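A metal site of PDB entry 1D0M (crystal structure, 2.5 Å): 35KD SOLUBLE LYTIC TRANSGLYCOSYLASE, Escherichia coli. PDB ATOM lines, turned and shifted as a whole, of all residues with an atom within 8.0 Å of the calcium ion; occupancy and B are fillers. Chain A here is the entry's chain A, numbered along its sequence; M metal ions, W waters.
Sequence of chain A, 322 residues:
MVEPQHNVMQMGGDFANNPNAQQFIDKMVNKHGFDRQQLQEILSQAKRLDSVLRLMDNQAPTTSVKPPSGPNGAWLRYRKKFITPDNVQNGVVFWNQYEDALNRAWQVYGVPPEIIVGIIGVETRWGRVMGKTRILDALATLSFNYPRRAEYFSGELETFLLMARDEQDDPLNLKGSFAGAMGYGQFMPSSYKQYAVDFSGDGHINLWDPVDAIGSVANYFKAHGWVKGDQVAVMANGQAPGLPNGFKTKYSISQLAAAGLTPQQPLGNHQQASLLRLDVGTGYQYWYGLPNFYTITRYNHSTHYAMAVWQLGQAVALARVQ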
ATOM      1  N   GLU A 167     -33.096   9.742  10.290  1.00  0.00           N
ATOM      2  CA  GLU A 167     -31.857  10.276  10.853  1.00  0.00           C
ATOM      3  C   GLU A 167     -31.909  10.464  12.372  1.00  0.00           C
ATOM      4  O   GLU A 167     -31.051  11.138  12.949  1.00  0.00           O
ATOM      5  CB  GLU A 167     -31.492  11.607  10.187  1.00  0.00           C
ATOM      6  CG  GLU A 167     -31.218  11.522   8.691  1.00  0.00           C
ATOM      7  CD  GLU A 167     -30.050  10.604   8.332  1.00  0.00           C
ATOM      8  OE1 GLU A 167     -29.160  10.397   9.187  1.00  0.00           O
ATOM      9  OE2 GLU A 167     -30.038  10.091   7.192  1.00  0.00           O
ATOM     10  N   VAL A 197     -26.165  13.504   0.318  1.00  0.00           N
ATOM     11  CA  VAL A 197     -25.326  12.327   0.414  1.00  0.00           C
ATOM     12  C   VAL A 197     -24.466  12.304   1.685  1.00  0.00           C
ATOM     13  O   VAL A 197     -24.130  13.344   2.242  1.00  0.00           O
ATOM     14  CB  VAL A 197     -24.368  12.193  -0.830  1.00  0.00           C
ATOM     15  CG1 VAL A 197     -25.169  11.941  -2.106  1.00  0.00           C
ATOM     16  CG2 VAL A 197     -23.524  13.433  -0.983  1.00  0.00           C
ATOM     17  N   ASP A 198     -24.163  11.104   2.164  1.00  0.00           N
ATOM     18  CA  ASP A 198     -23.310  10.930   3.336  1.00  0.00           C
ATOM     19  C   ASP A 198     -21.866  11.142   2.885  1.00  0.00           C
ATOM     20  O   ASP A 198     -21.076  10.189   2.840  1.00  0.00           O
ATOM     21  CB  ASP A 198     -23.508   9.526   3.899  1.00  0.00           C
ATOM     22  CG  ASP A 198     -22.502   9.181   4.976  1.00  0.00           C
ATOM     23  OD1 ASP A 198     -21.940  10.095   5.610  1.00  0.00           O
ATOM     24  OD2 ASP A 198     -22.248   7.972   5.178  1.00  0.00           O
ATOM     25  N   PHE A 199     -21.500  12.372   2.587  1.00  0.00           N
ATOM     26  CA  PHE A 199     -20.150  12.637   2.102  1.00  0.00           C
ATOM     27  C   PHE A 199     -19.049  12.426   3.125  1.00  0.00           C
ATOM     28  O   PHE A 199     -17.895  12.208   2.749  1.00  0.00           O
ATOM     29  CB  PHE A 199     -20.058  14.048   1.518  1.00  0.00           C
ATOM     30  CG  PHE A 199     -19.070  14.146   0.387  1.00  0.00           C
ATOM     31  CD1 PHE A 199     -19.188  13.329  -0.724  1.00  0.00           C
ATOM     32  CD2 PHE A 199     -18.023  15.055   0.454  1.00  0.00           C
ATOM     33  CE1 PHE A 199     -18.280  13.402  -1.755  1.00  0.00           C
ATOM     34  CE2 PHE A 199     -17.097  15.134  -0.572  1.00  0.00           C
ATOM     35  CZ  PHE A 199     -17.227  14.313  -1.676  1.00  0.00           C
ATOM     36  N   SER A 200     -19.387  12.478   4.411  1.00  0.00           N
ATOM     37  CA  SER A 200     -18.421  12.287   5.489  1.00  0.00           C
ATOM     38  C   SER A 200     -18.128  10.819   5.764  1.00  0.00           C
ATOM     39  O   SER A 200     -17.111  10.504   6.407  1.00  0.00           O
ATOM     40  CB  SER A 200     -18.878  12.973   6.773  1.00  0.00           C
ATOM     41  OG  SER A 200     -19.918  12.242   7.384  1.00  0.00           O
ATOM     42  N   GLY A 201     -19.036   9.941   5.344  1.00  0.00           N
ATOM     43  CA  GLY A 201     -18.851   8.510   5.506  1.00  0.00           C
ATOM     44  C   GLY A 201     -19.196   7.866   6.834  1.00  0.00           C
ATOM     45  O   GLY A 201     -18.764   6.736   7.086  1.00  0.00           O
ATOM     46  N   ASP A 202     -19.952   8.554   7.683  1.00  0.00           N
ATOM     47  CA  ASP A 202     -20.319   8.007   8.982  1.00  0.00           C
ATOM     48  C   ASP A 202     -21.634   7.212   8.982  1.00  0.00           C
ATOM     49  O   ASP A 202     -22.075   6.713  10.022  1.00  0.00           O
ATOM     50  CB  ASP A 202     -20.327   9.109  10.059  1.00  0.00           C
ATOM     51  CG  ASP A 202     -21.474  10.092   9.917  1.00  0.00           C
ATOM     52  OD1 ASP A 202     -22.033  10.246   8.810  1.00  0.00           O
ATOM     53  OD2 ASP A 202     -21.818  10.738  10.928  1.00  0.00           O
ATOM     54  N   GLY A 203     -22.229   7.081   7.798  1.00  0.00           N
ATOM     55  CA  GLY A 203     -23.477   6.359   7.656  1.00  0.00           C
ATOM     56  C   GLY A 203     -24.745   7.179   7.778  1.00  0.00           C
ATOM     57  O   GLY A 203     -25.840   6.694   7.503  1.00  0.00           O
ATOM     58  N   HIS A 204     -24.603   8.448   8.160  1.00  0.00           N
ATOM     59  CA  HIS A 204     -25.746   9.341   8.335  1.00  0.00           C
ATOM     60  C   HIS A 204     -25.648  10.615   7.532  1.00  0.00           C
ATOM     61  O   HIS A 204     -24.598  11.229   7.480  1.00  0.00           O
ATOM     62  CB  HIS A 204     -25.896   9.686   9.828  1.00  0.00           C
ATOM     63  CG  HIS A 204     -26.208   8.501  10.691  1.00  0.00           C
ATOM     64  ND1 HIS A 204     -27.486   8.206  11.121  1.00  0.00           N
ATOM     65  CD2 HIS A 204     -25.412   7.524  11.190  1.00  0.00           C
ATOM     66  CE1 HIS A 204     -27.451   7.100  11.853  1.00  0.00           C
ATOM     67  NE2 HIS A 204     -26.205   6.675  11.906  1.00  0.00           N
ATOM     68  N   ILE A 205     -26.745  11.010   6.883  1.00  0.00           N
ATOM     69  CA  ILE A 205     -26.782  12.230   6.076  1.00  0.00           C
ATOM     70  C   ILE A 205     -27.261  13.387   6.955  1.00  0.00           C
ATOM     71  O   ILE A 205     -28.462  13.547   7.196  1.00  0.00           O
ATOM     72  CB  ILE A 205     -27.744  12.084   4.886  1.00  0.00           C
ATOM     73  CG1 ILE A 205     -27.381  10.857   4.062  1.00  0.00           C
ATOM     74  CG2 ILE A 205     -27.725  13.342   4.037  1.00  0.00           C
ATOM     75  CD1 ILE A 205     -28.436  10.483   3.044  1.00  0.00           C
ATOM     76  N   ASN A 206     -26.300  14.177   7.436  1.00  0.00           N
ATOM     77  CA  ASN A 206     -26.547  15.315   8.298  1.00  0.00           C
ATOM     78  C   ASN A 206     -26.335  16.606   7.499  1.00  0.00           C
ATOM     79  O   ASN A 206     -25.254  16.835   6.962  1.00  0.00           O
ATOM     80  CB  ASN A 206     -25.545  15.264   9.462  1.00  0.00           C
ATOM     81  CG  ASN A 206     -25.868  16.222  10.569  1.00  0.00           C
ATOM     82  OD1 ASN A 206     -26.851  16.943  10.526  1.00  0.00           O
ATOM     83  ND2 ASN A 206     -25.034  16.220  11.593  1.00  0.00           N
ATOM     84  N   LEU A 207     -27.364  17.438   7.420  1.00  0.00           N
ATOM     85  CA  LEU A 207     -27.259  18.694   6.681  1.00  0.00           C
ATOM     86  C   LEU A 207     -26.477  19.766   7.426  1.00  0.00           C
ATOM     87  O   LEU A 207     -26.129  20.798   6.844  1.00  0.00           O
ATOM     88  CB  LEU A 207     -28.650  19.217   6.331  1.00  0.00           C
ATOM     89  CG  LEU A 207     -29.399  18.333   5.330  1.00  0.00           C
ATOM     90  CD1 LEU A 207     -30.848  18.787   5.229  1.00  0.00           C
ATOM     91  CD2 LEU A 207     -28.695  18.379   3.973  1.00  0.00           C
ATOM     92  N   ASP A 209     -23.585  19.049   8.940  1.00  0.00           N
ATOM     93  CA  ASP A 209     -22.209  18.569   8.922  1.00  0.00           C
ATOM     94  C   ASP A 209     -21.614  19.244   7.671  1.00  0.00           C
ATOM     95  O   ASP A 209     -22.098  19.043   6.556  1.00  0.00           O
ATOM     96  CB  ASP A 209     -22.210  17.043   8.769  1.00  0.00           C
ATOM     97  CG  ASP A 209     -20.817  16.434   8.860  1.00  0.00           C
ATOM     98  OD1 ASP A 209     -19.881  16.931   8.198  1.00  0.00           O
ATOM     99  OD2 ASP A 209     -20.662  15.420   9.572  1.00  0.00           O
ATOM    100  N   VAL A 211     -19.016  18.690   5.875  1.00  0.00           N
ATOM    101  CA  VAL A 211     -18.561  17.755   4.851  1.00  0.00           C
ATOM    102  C   VAL A 211     -19.705  17.175   4.009  1.00  0.00           C
ATOM    103  O   VAL A 211     -19.585  17.054   2.788  1.00  0.00           O
ATOM    104  CB  VAL A 211     -17.681  16.638   5.468  1.00  0.00           C
ATOM    105  CG1 VAL A 211     -17.277  15.612   4.421  1.00  0.00           C
ATOM    106  CG2 VAL A 211     -16.444  17.267   6.112  1.00  0.00           C
ATOM    107  N   ASP A 212     -20.826  16.871   4.675  1.00  0.00           N
ATOM    108  CA  ASP A 212     -22.012  16.332   4.023  1.00  0.00           C
ATOM    109  C   ASP A 212     -22.658  17.385   3.124  1.00  0.00           C
ATOM    110  O   ASP A 212     -23.144  17.068   2.030  1.00  0.00           O
ATOM    111  CB  ASP A 212     -23.047  15.923   5.071  1.00  0.00           C
ATOM    112  CG  ASP A 212     -22.783  14.564   5.661  1.00  0.00           C
ATOM    113  OD1 ASP A 212     -21.644  14.049   5.558  1.00  0.00           O
ATOM    114  OD2 ASP A 212     -23.719  13.993   6.232  1.00  0.00           O
ATOM    115  N   ALA A 213     -22.713  18.613   3.612  1.00  0.00           N
ATOM    116  CA  ALA A 213     -23.280  19.735   2.870  1.00  0.00           C
ATOM    117  C   ALA A 213     -22.476  19.951   1.610  1.00  0.00           C
ATOM    118  O   ALA A 213     -23.056  20.151   0.553  1.00  0.00           O
ATOM    119  CB  ALA A 213     -23.239  20.988   3.713  1.00  0.00           C
HETATM  120 CA    CA M   1     -22.423  12.100   7.168  1.00  0.00          CA
HETATM  121  O   HOH W   1     -22.533  13.297   9.438  1.00  0.00           O
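Water W1 lies within hydrogen-bond range of the side-chain carboxylate (OD2) of Asp 209 (2.8 Å) and the side-chain carboxylate (OD2) of Asp 202 (3.0 Å).
The calcium ion is bound by O of His 204 (2.4 Å). OD2 of Asp 212 is bound to the calcium ion, 2.5 Å away. OD1 of Asp 202 is bound to the calcium ion. The calcium ion is bound by OG of Ser 200 (2.5 Å). Water W1 binds the calcium ion, 2.6 Å away. The side-chain carboxylate (OD1) of Asp 198 binds the calcium ion, at 2.6 Å. OD1 of Asp 212 is bound to the calcium ion (2.6 Å). The calcium ion has seven donor atoms within binding distance.
A ring nitrogen (ND1) of His 204 lies within hydrogen-bond range of the side-chain carboxylate (OE1) of Glu 167. OD2 of Asp 212 sits close to N of Asn 206, at 2.9 Å. OD1 of Asp 212 sits close to N of Phe 199 (3.4 Å). OD1 of Asp 198 sits close to N of Gly 201. The side-chain carboxylate (OD2) of Asp 198 is in hydrogen-bond range of the backbone NH (N) of Gly 203.
Within 4 Å of the calcium ion: Asp 198, Ser 200, Asp 202, His 204 and Asp 212.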
